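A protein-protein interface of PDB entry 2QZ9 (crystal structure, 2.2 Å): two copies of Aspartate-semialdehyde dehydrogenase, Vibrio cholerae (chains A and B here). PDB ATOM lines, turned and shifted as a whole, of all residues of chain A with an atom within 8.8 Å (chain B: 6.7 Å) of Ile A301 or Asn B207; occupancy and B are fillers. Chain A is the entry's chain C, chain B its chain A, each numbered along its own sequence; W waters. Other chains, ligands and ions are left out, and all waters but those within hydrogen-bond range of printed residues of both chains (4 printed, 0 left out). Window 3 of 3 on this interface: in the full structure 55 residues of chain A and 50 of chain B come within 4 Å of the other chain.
NH2 of Arg A296 lies within hydrogen-bond range of O of Gly B208 (2.9 Å). The backbone carbonyl oxygen (O) of Asn A299 lies close to the side-chain hydroxyl (OH) of Tyr B209 (3.5 Å). N of Ile A301 lies within hydrogen-bond range of OH of Tyr B209, at 3.3 Å. The side-chain hydroxyl (OH) of Tyr B209 lies within hydrogen-bond range of the side-chain amide nitrogen (ND2) of Asn A308 (3.0 Å). OE1 of Glu B213 lies within salt-bridge range of NH2 of Arg A296, at 2.8 Å. The guanidinium group (NH2) of Arg A298 lies within salt-bridge range of the side-chain carboxylate (OE1) of Glu B213, at 3.7 Å. The side-chain amide oxygen (OD1) of Asn B232 lies close to the side-chain carboxylate (OD2) of Asp A300, at 3.1 Å. The side-chain amide nitrogen of Asn A308 lies close to the side-chain amide nitrogen of Asn B232, 2.7 Å away. The guanidinium group (NH2) of Arg A298 is in hydrogen-bond range of the backbone carbonyl oxygen (O) of Pro B233 (3.0 Å).
OD1 of Asn B207 sits at hydrogen-bond distance from N of Tyr B209, 3.1 Å away. The side-chain amide nitrogen (ND2) of Asn B232 is in hydrogen-bond range of the side-chain hydroxyl (OH) of Tyr B209 (2.7 Å). N of Ala A258 sits at hydrogen-bond distance from OD1 of Asn A299. O of Arg A298 lies within hydrogen-bond range of N of Asn A308, at 2.9 Å. OD1 of Asp A300 sits at hydrogen-bond distance from OG of Ser A302 (2.6 Å). The backbone carbonyl oxygen of Gly A306 is in hydrogen-bond range of the backbone NH of Asp A300 (3.0 Å).
Among the printed residues, pairs that only touch across the chains: Arg A296 with Phe B204, Arg A296 with Tyr B209, Arg A298 with Asn B207, Arg A298 with Gly B208, Arg A298 with Tyr B209, Asp A300 with Tyr B209, Ile A301 with Asn B207, Ile A301 with Met B214, Ser A302 with Met B230, Ser A302 with Val B231 and Ser A302 with Asn B232.
Val A297 touches none of the printed residues of chain B. Printed residues of chain B within 4 Å of Asn A299: Tyr B209 (3.3 Å). Of the printed residues of chain B, Asp A300 touches Tyr B209 (3.3 Å) and Asn B232 (3.1 Å). Of chain B, only Asn B207, Tyr B209 and Met B214 come within 4 Å of Ile A301. Of the printed residues of chain B, Ser A302 touches Met B230, Val B231 and Asn B232. His A304 touches none of the printed residues of chain B. Printed residues of chain A within 4 Å of Phe B204: Arg A296 (3.5 Å). Asn B207 touches just these residues of chain A: Arg A298 (3.7 Å) and Ile A301 (3.95 Å). Gly B208 touches just these residues of chain A: Arg A296 and Arg A298. Printed residues of chain A within 4 Å of Pro B233: Arg A298. The nearest residue of chain B that does not touch Ile A301 is Val B217 (4.2 Å). The nearest residue of chain A that does not touch Asn B207 is Asn A299 (4.6 Å). The nearest printed residue of chain B that does not touch Asn A299 is Asn B207 (4.6 Å).
Hydrophobic or aromatic side chains of chain B that line the printed part of chain A: Phe B204, Tyr B209, Met B214 and Met B230. Among the printed residues, 20 pairs touch across the chains. Among the printed residues, Asp or Glu carboxylates within 4 Å of a Lys or Arg side-chain nitrogen of the other chain: Arg A296 with Glu B213 (2.8 Å) and Arg A298 with Glu B213 (3.7 Å).
No position is printed for both chains.
Water W4 bridges O of Asn B207 and O of Asn A299. Water W1 bridges O of Gly B208 (2.6 Å) and NE of Arg A296 (2.7 Å). Water W3 lies within hydrogen-bond range of the side-chain carboxylate of Glu B213 (2.7 Å), the side-chain hydroxyl of Thr B210 (2.9 Å) and the guanidinium group of Arg A296 (3.4 Å). Water W2 lies within hydrogen-bond range of N of Asn A299 (3.1 Å) and O of Asn B207 (3.2 Å).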
ATOM      1  N   ALA A 258      38.395  28.645 -10.433  1.00  0.00           N
ATOM      2  CA  ALA A 258      38.532  27.556 -11.398  1.00  0.00           C
ATOM      3  C   ALA A 258      39.960  27.417 -11.924  1.00  0.00           C
ATOM      4  O   ALA A 258      40.405  26.303 -12.224  1.00  0.00           O
ATOM      5  CB  ALA A 258      37.547  27.724 -12.548  1.00  0.00           C
ATOM      6  N   ARG A 296      35.359  21.178 -18.616  1.00  0.00           N
ATOM      7  CA  ARG A 296      34.357  22.199 -18.280  1.00  0.00           C
ATOM      8  C   ARG A 296      34.524  22.794 -16.883  1.00  0.00           C
ATOM      9  O   ARG A 296      33.542  23.210 -16.281  1.00  0.00           O
ATOM     10  CB  ARG A 296      32.924  21.665 -18.441  1.00  0.00           C
ATOM     11  CG  ARG A 296      32.570  20.996 -19.786  1.00  0.00           C
ATOM     12  CD  ARG A 296      32.108  21.977 -20.873  1.00  0.00           C
ATOM     13  NE  ARG A 296      31.608  23.249 -20.339  1.00  0.00           N
ATOM     14  CZ  ARG A 296      30.330  23.614 -20.284  1.00  0.00           C
ATOM     15  NH1 ARG A 296      29.355  22.813 -20.723  1.00  0.00           N
ATOM     16  NH2 ARG A 296      30.025  24.808 -19.782  1.00  0.00           N
ATOM     17  N   VAL A 297      35.753  22.828 -16.366  1.00  0.00           N
ATOM     18  CA  VAL A 297      36.004  23.393 -15.037  1.00  0.00           C
ATOM     19  C   VAL A 297      35.816  24.906 -15.099  1.00  0.00           C
ATOM     20  O   VAL A 297      36.465  25.594 -15.899  1.00  0.00           O
ATOM     21  CB  VAL A 297      37.400  23.034 -14.477  1.00  0.00           C
ATOM     22  CG1 VAL A 297      37.498  23.408 -13.016  1.00  0.00           C
ATOM     23  CG2 VAL A 297      37.686  21.537 -14.620  1.00  0.00           C
ATOM     24  N   ARG A 298      34.900  25.406 -14.278  1.00  0.00           N
ATOM     25  CA  ARG A 298      34.506  26.811 -14.314  1.00  0.00           C
ATOM     26  C   ARG A 298      33.854  27.220 -12.996  1.00  0.00           C
ATOM     27  O   ARG A 298      33.223  26.399 -12.327  1.00  0.00           O
ATOM     28  CB  ARG A 298      33.550  27.079 -15.499  1.00  0.00           C
ATOM     29  CG  ARG A 298      32.137  26.461 -15.378  1.00  0.00           C
ATOM     30  CD  ARG A 298      31.547  26.185 -16.744  1.00  0.00           C
ATOM     31  NE  ARG A 298      30.146  25.765 -16.692  1.00  0.00           N
ATOM     32  CZ  ARG A 298      29.722  24.500 -16.596  1.00  0.00           C
ATOM     33  NH1 ARG A 298      30.588  23.496 -16.521  1.00  0.00           N
ATOM     34  NH2 ARG A 298      28.424  24.233 -16.556  1.00  0.00           N
ATOM     35  N   ASN A 299      34.020  28.492 -12.628  1.00  0.00           N
ATOM     36  CA  ASN A 299      33.339  29.055 -11.475  1.00  0.00           C
ATOM     37  C   ASN A 299      31.834  28.975 -11.681  1.00  0.00           C
ATOM     38  O   ASN A 299      31.325  29.190 -12.778  1.00  0.00           O
ATOM     39  CB  ASN A 299      33.728  30.514 -11.261  1.00  0.00           C
ATOM     40  CG  ASN A 299      35.184  30.691 -10.882  1.00  0.00           C
ATOM     41  OD1 ASN A 299      35.831  29.767 -10.403  1.00  0.00           O
ATOM     42  ND2 ASN A 299      35.703  31.903 -11.080  1.00  0.00           N
ATOM     43  N   ASP A 300      31.141  28.657 -10.601  1.00  0.00           N
ATOM     44  CA  ASP A 300      29.701  28.615 -10.563  1.00  0.00           C
ATOM     45  C   ASP A 300      29.212  30.058 -10.360  1.00  0.00           C
ATOM     46  O   ASP A 300      29.443  30.659  -9.309  1.00  0.00           O
ATOM     47  CB  ASP A 300      29.301  27.704  -9.396  1.00  0.00           C
ATOM     48  CG  ASP A 300      27.810  27.628  -9.163  1.00  0.00           C
ATOM     49  OD1 ASP A 300      27.029  28.293  -9.865  1.00  0.00           O
ATOM     50  OD2 ASP A 300      27.422  26.884  -8.239  1.00  0.00           O
ATOM     51  N   ILE A 301      28.558  30.610 -11.377  1.00  0.00           N
ATOM     52  CA  ILE A 301      28.018  31.973 -11.306  1.00  0.00           C
ATOM     53  C   ILE A 301      26.819  32.124 -10.360  1.00  0.00           C
ATOM     54  O   ILE A 301      26.429  33.237 -10.029  1.00  0.00           O
ATOM     55  CB  ILE A 301      27.651  32.500 -12.705  1.00  0.00           C
ATOM     56  CG1 ILE A 301      26.636  31.567 -13.383  1.00  0.00           C
ATOM     57  CG2 ILE A 301      28.921  32.650 -13.547  1.00  0.00           C
ATOM     58  CD1 ILE A 301      26.178  32.035 -14.757  1.00  0.00           C
ATOM     59  N   SER A 302      26.246  31.002  -9.928  1.00  0.00           N
ATOM     60  CA  SER A 302      25.069  30.999  -9.074  1.00  0.00           C
ATOM     61  C   SER A 302      25.395  30.952  -7.570  1.00  0.00           C
ATOM     62  O   SER A 302      24.500  31.005  -6.738  1.00  0.00           O
ATOM     63  CB  SER A 302      24.155  29.830  -9.455  1.00  0.00           C
ATOM     64  OG  SER A 302      24.614  28.605  -8.899  1.00  0.00           O
ATOM     65  N   HIS A 303      26.677  30.873  -7.235  1.00  0.00           N
ATOM     66  CA  HIS A 303      27.132  30.650  -5.855  1.00  0.00           C
ATOM     67  C   HIS A 303      28.484  31.328  -5.612  1.00  0.00           C
ATOM     68  O   HIS A 303      29.285  31.456  -6.543  1.00  0.00           O
ATOM     69  CB  HIS A 303      27.265  29.146  -5.603  1.00  0.00           C
ATOM     70  CG  HIS A 303      27.240  28.771  -4.156  1.00  0.00           C
ATOM     71  ND1 HIS A 303      28.383  28.660  -3.397  1.00  0.00           N
ATOM     72  CD2 HIS A 303      26.210  28.479  -3.327  1.00  0.00           C
ATOM     73  CE1 HIS A 303      28.061  28.314  -2.163  1.00  0.00           C
ATOM     74  NE2 HIS A 303      26.748  28.197  -2.094  1.00  0.00           N
ATOM     75  N   HIS A 304      28.746  31.750  -4.374  1.00  0.00           N
ATOM     76  CA  HIS A 304      30.007  32.466  -4.057  1.00  0.00           C
ATOM     77  C   HIS A 304      31.249  31.578  -4.094  1.00  0.00           C
ATOM     78  O   HIS A 304      32.319  32.011  -4.542  1.00  0.00           O
ATOM     79  CB  HIS A 304      29.918  33.255  -2.741  1.00  0.00           C
ATOM     80  CG  HIS A 304      29.389  32.464  -1.585  1.00  0.00           C
ATOM     81  ND1 HIS A 304      28.051  32.440  -1.251  1.00  0.00           N
ATOM     82  CD2 HIS A 304      30.020  31.687  -0.669  1.00  0.00           C
ATOM     83  CE1 HIS A 304      27.877  31.668  -0.192  1.00  0.00           C
ATOM     84  NE2 HIS A 304      29.055  31.198   0.179  1.00  0.00           N
ATOM     85  N   SER A 305      31.101  30.331  -3.663  1.00  0.00           N
ATOM     86  CA  SER A 305      32.190  29.378  -3.731  1.00  0.00           C
ATOM     87  C   SER A 305      31.730  28.057  -4.347  1.00  0.00           C
ATOM     88  O   SER A 305      31.686  27.030  -3.674  1.00  0.00           O
ATOM     89  CB  SER A 305      32.774  29.154  -2.336  1.00  0.00           C
ATOM     90  OG  SER A 305      31.745  28.826  -1.422  1.00  0.00           O
ATOM     91  N   GLY A 306      31.400  28.096  -5.635  1.00  0.00           N
ATOM     92  CA  GLY A 306      30.981  26.916  -6.366  1.00  0.00           C
ATOM     93  C   GLY A 306      31.913  26.644  -7.534  1.00  0.00           C
ATOM     94  O   GLY A 306      32.425  27.576  -8.147  1.00  0.00           O
ATOM     95  N   ILE A 307      32.140  25.366  -7.834  1.00  0.00           N
ATOM     96  CA  ILE A 307      32.896  24.953  -9.031  1.00  0.00           C
ATOM     97  C   ILE A 307      32.057  23.929  -9.813  1.00  0.00           C
ATOM     98  O   ILE A 307      31.502  23.018  -9.211  1.00  0.00           O
ATOM     99  CB  ILE A 307      34.283  24.351  -8.646  1.00  0.00           C
ATOM    100  CG1 ILE A 307      35.164  25.380  -7.902  1.00  0.00           C
ATOM    101  CG2 ILE A 307      35.018  23.782  -9.871  1.00  0.00           C
ATOM    102  CD1 ILE A 307      35.760  26.475  -8.787  1.00  0.00           C
ATOM    103  N   ASN A 308      31.936  24.093 -11.130  1.00  0.00           N
ATOM    104  CA  ASN A 308      31.292  23.079 -11.972  1.00  0.00           C
ATOM    105  C   ASN A 308      32.355  22.335 -12.758  1.00  0.00           C
ATOM    106  O   ASN A 308      33.350  22.919 -13.166  1.00  0.00           O
ATOM    107  CB  ASN A 308      30.316  23.671 -12.991  1.00  0.00           C
ATOM    108  CG  ASN A 308      29.160  24.419 -12.366  1.00  0.00           C
ATOM    109  OD1 ASN A 308      29.004  24.500 -11.143  1.00  0.00           O
ATOM    110  ND2 ASN A 308      28.331  24.976 -13.223  1.00  0.00           N
ATOM    111  N   PHE B 204      31.106  28.551 -26.508  1.00  0.00           N
ATOM    112  CA  PHE B 204      31.508  28.923 -25.163  1.00  0.00           C
ATOM    113  C   PHE B 204      31.536  30.430 -24.959  1.00  0.00           C
ATOM    114  O   PHE B 204      31.619  31.201 -25.923  1.00  0.00           O
ATOM    115  CB  PHE B 204      32.878  28.329 -24.843  1.00  0.00           C
ATOM    116  CG  PHE B 204      32.863  26.834 -24.685  1.00  0.00           C
ATOM    117  CD1 PHE B 204      33.392  26.011 -25.677  1.00  0.00           C
ATOM    118  CD2 PHE B 204      32.309  26.247 -23.546  1.00  0.00           C
ATOM    119  CE1 PHE B 204      33.377  24.621 -25.533  1.00  0.00           C
ATOM    120  CE2 PHE B 204      32.284  24.864 -23.390  1.00  0.00           C
ATOM    121  CZ  PHE B 204      32.823  24.047 -24.379  1.00  0.00           C
ATOM    122  N   MET B 205      31.476  30.835 -23.693  1.00  0.00           N
ATOM    123  CA  MET B 205      31.476  32.241 -23.302  1.00  0.00           C
ATOM    124  C   MET B 205      32.693  32.483 -22.435  1.00  0.00           C
ATOM    125  O   MET B 205      33.360  31.532 -22.030  1.00  0.00           O
ATOM    126  CB  MET B 205      30.209  32.581 -22.509  1.00  0.00           C
ATOM    127  CG  MET B 205      28.909  32.157 -23.182  1.00  0.00           C
ATOM    128  SD  MET B 205      28.110  33.431 -24.177  1.00  0.00           S
ATOM    129  CE  MET B 205      27.355  34.437 -22.906  1.00  0.00           C
ATOM    130  N   ASP B 206      32.970  33.753 -22.144  1.00  0.00           N
ATOM    131  CA  ASP B 206      34.125  34.153 -21.331  1.00  0.00           C
ATOM    132  C   ASP B 206      34.157  33.467 -19.976  1.00  0.00           C
ATOM    133  O   ASP B 206      35.229  33.313 -19.376  1.00  0.00           O
ATOM    134  CB  ASP B 206      34.136  35.676 -21.101  1.00  0.00           C
ATOM    135  CG  ASP B 206      34.032  36.484 -22.397  1.00  0.00           C
ATOM    136  OD1 ASP B 206      34.582  36.056 -23.449  1.00  0.00           O
ATOM    137  OD2 ASP B 206      33.400  37.569 -22.354  1.00  0.00           O
ATOM    138  N   ASN B 207      32.983  33.071 -19.485  1.00  0.00           N
ATOM    139  CA  ASN B 207      32.877  32.542 -18.125  1.00  0.00           C
ATOM    140  C   ASN B 207      32.949  31.003 -17.988  1.00  0.00           C
ATOM    141  O   ASN B 207      32.856  30.471 -16.886  1.00  0.00           O
ATOM    142  CB  ASN B 207      31.660  33.135 -17.399  1.00  0.00           C
ATOM    143  CG  ASN B 207      30.332  32.705 -17.997  1.00  0.00           C
ATOM    144  OD1 ASN B 207      30.270  31.914 -18.947  1.00  0.00           O
ATOM    145  ND2 ASN B 207      29.256  33.230 -17.442  1.00  0.00           N
ATOM    146  N   GLY B 208      33.128  30.307 -19.106  1.00  0.00           N
ATOM    147  CA  GLY B 208      33.182  28.846 -19.109  1.00  0.00           C
ATOM    148  C   GLY B 208      31.880  28.188 -19.516  1.00  0.00           C
ATOM    149  O   GLY B 208      31.875  27.047 -19.977  1.00  0.00           O
ATOM    150  N   TYR B 209      30.770  28.903 -19.346  1.00  0.00           N
ATOM    151  CA  TYR B 209      29.457  28.389 -19.721  1.00  0.00           C
ATOM    152  C   TYR B 209      29.254  28.543 -21.211  1.00  0.00           C
ATOM    153  O   TYR B 209      29.971  29.311 -21.854  1.00  0.00           O
ATOM    154  CB  TYR B 209      28.338  29.125 -18.977  1.00  0.00           C
ATOM    155  CG  TYR B 209      28.265  28.810 -17.501  1.00  0.00           C
ATOM    156  CD1 TYR B 209      29.139  29.408 -16.609  1.00  0.00           C
ATOM    157  CD2 TYR B 209      27.316  27.923 -16.998  1.00  0.00           C
ATOM    158  CE1 TYR B 209      29.090  29.128 -15.255  1.00  0.00           C
ATOM    159  CE2 TYR B 209      27.255  27.637 -15.628  1.00  0.00           C
ATOM    160  CZ  TYR B 209      28.149  28.252 -14.771  1.00  0.00           C
ATOM    161  OH  TYR B 209      28.121  28.010 -13.423  1.00  0.00           O
ATOM    162  N   THR B 210      28.272  27.837 -21.758  1.00  0.00           N
ATOM    163  CA  THR B 210      27.947  28.000 -23.168  1.00  0.00           C
ATOM    164  C   THR B 210      26.788  28.967 -23.282  1.00  0.00           C
ATOM    165  O   THR B 210      26.184  29.331 -22.270  1.00  0.00           O
ATOM    166  CB  THR B 210      27.572  26.671 -23.853  1.00  0.00           C
ATOM    167  OG1 THR B 210      26.364  26.166 -23.282  1.00  0.00           O
ATOM    168  CG2 THR B 210      28.681  25.648 -23.703  1.00  0.00           C
ATOM    169  N   GLU B 213      23.567  27.450 -21.994  1.00  0.00           N
ATOM    170  CA  GLU B 213      23.578  27.518 -20.538  1.00  0.00           C
ATOM    171  C   GLU B 213      23.282  28.952 -20.089  1.00  0.00           C
ATOM    172  O   GLU B 213      22.414  29.183 -19.239  1.00  0.00           O
ATOM    173  CB  GLU B 213      24.914  27.004 -19.997  1.00  0.00           C
ATOM    174  CG  GLU B 213      25.165  25.532 -20.339  1.00  0.00           C
ATOM    175  CD  GLU B 213      26.583  25.052 -20.083  1.00  0.00           C
ATOM    176  OE1 GLU B 213      27.472  25.858 -19.734  1.00  0.00           O
ATOM    177  OE2 GLU B 213      26.821  23.832 -20.232  1.00  0.00           O
ATOM    178  N   MET B 214      23.977  29.915 -20.696  1.00  0.00           N
ATOM    179  CA  MET B 214      23.729  31.328 -20.409  1.00  0.00           C
ATOM    180  C   MET B 214      22.311  31.793 -20.740  1.00  0.00           C
ATOM    181  O   MET B 214      21.786  32.663 -20.053  1.00  0.00           O
ATOM    182  CB  MET B 214      24.806  32.238 -21.027  1.00  0.00           C
ATOM    183  CG  MET B 214      26.145  32.220 -20.250  1.00  0.00           C
ATOM    184  SD  MET B 214      25.939  32.173 -18.438  1.00  0.00           S
ATOM    185  CE  MET B 214      25.279  33.831 -18.156  1.00  0.00           C
ATOM    186  N   VAL B 217      19.953  30.798 -17.840  1.00  0.00           N
ATOM    187  CA  VAL B 217      20.152  31.838 -16.821  1.00  0.00           C
ATOM    188  C   VAL B 217      19.343  33.111 -17.114  1.00  0.00           C
ATOM    189  O   VAL B 217      18.433  33.456 -16.364  1.00  0.00           O
ATOM    190  CB  VAL B 217      21.654  32.185 -16.667  1.00  0.00           C
ATOM    191  CG1 VAL B 217      21.849  33.372 -15.717  1.00  0.00           C
ATOM    192  CG2 VAL B 217      22.421  30.969 -16.183  1.00  0.00           C
ATOM    193  N   MET B 230      19.166  32.406  -8.694  1.00  0.00           N
ATOM    194  CA  MET B 230      20.432  31.922  -9.186  1.00  0.00           C
ATOM    195  C   MET B 230      20.192  30.679 -10.034  1.00  0.00           C
ATOM    196  O   MET B 230      19.409  29.821  -9.667  1.00  0.00           O
ATOM    197  CB  MET B 230      21.371  31.664  -8.010  1.00  0.00           C
ATOM    198  CG  MET B 230      21.736  32.949  -7.203  1.00  0.00           C
ATOM    199  SD  MET B 230      22.573  34.222  -8.179  1.00  0.00           S
ATOM    200  CE  MET B 230      21.237  35.303  -8.665  1.00  0.00           C
ATOM    201  N   VAL B 231      20.833  30.615 -11.193  1.00  0.00           N
ATOM    202  CA  VAL B 231      20.624  29.498 -12.117  1.00  0.00           C
ATOM    203  C   VAL B 231      21.986  28.963 -12.531  1.00  0.00           C
ATOM    204  O   VAL B 231      22.823  29.712 -13.028  1.00  0.00           O
ATOM    205  CB  VAL B 231      19.779  29.900 -13.376  1.00  0.00           C
ATOM    206  CG1 VAL B 231      19.441  28.674 -14.227  1.00  0.00           C
ATOM    207  CG2 VAL B 231      18.504  30.638 -12.967  1.00  0.00           C
ATOM    208  N   ASN B 232      22.195  27.663 -12.328  1.00  0.00           N
ATOM    209  CA  ASN B 232      23.489  27.025 -12.604  1.00  0.00           C
ATOM    210  C   ASN B 232      23.305  25.823 -13.536  1.00  0.00           C
ATOM    211  O   ASN B 232      23.047  24.717 -13.074  1.00  0.00           O
ATOM    212  CB  ASN B 232      24.125  26.605 -11.279  1.00  0.00           C
ATOM    213  CG  ASN B 232      25.526  26.061 -11.435  1.00  0.00           C
ATOM    214  OD1 ASN B 232      26.007  25.337 -10.559  1.00  0.00           O
ATOM    215  ND2 ASN B 232      26.197  26.403 -12.537  1.00  0.00           N
ATOM    216  N   PRO B 233      23.381  26.048 -14.854  1.00  0.00           N
ATOM    217  CA  PRO B 233      23.187  24.965 -15.820  1.00  0.00           C
ATOM    218  C   PRO B 233      24.454  24.269 -16.333  1.00  0.00           C
ATOM    219  O   PRO B 233      25.510  24.886 -16.416  1.00  0.00           O
ATOM    220  CB  PRO B 233      22.472  25.672 -16.997  1.00  0.00           C
ATOM    221  CG  PRO B 233      22.523  27.187 -16.661  1.00  0.00           C
ATOM    222  CD  PRO B 233      23.541  27.335 -15.546  1.00  0.00           C
HETATM  223  O   HOH W   1      33.562  25.014 -19.769  1.00  0.00           O
HETATM  224  O   HOH W   2      35.425  30.046 -14.943  1.00  0.00           O
HETATM  225  O   HOH W   3      26.697  23.310 -22.854  1.00  0.00           O
HETATM  226  O   HOH W   4      32.290  31.203 -14.577  1.00  0.00           O
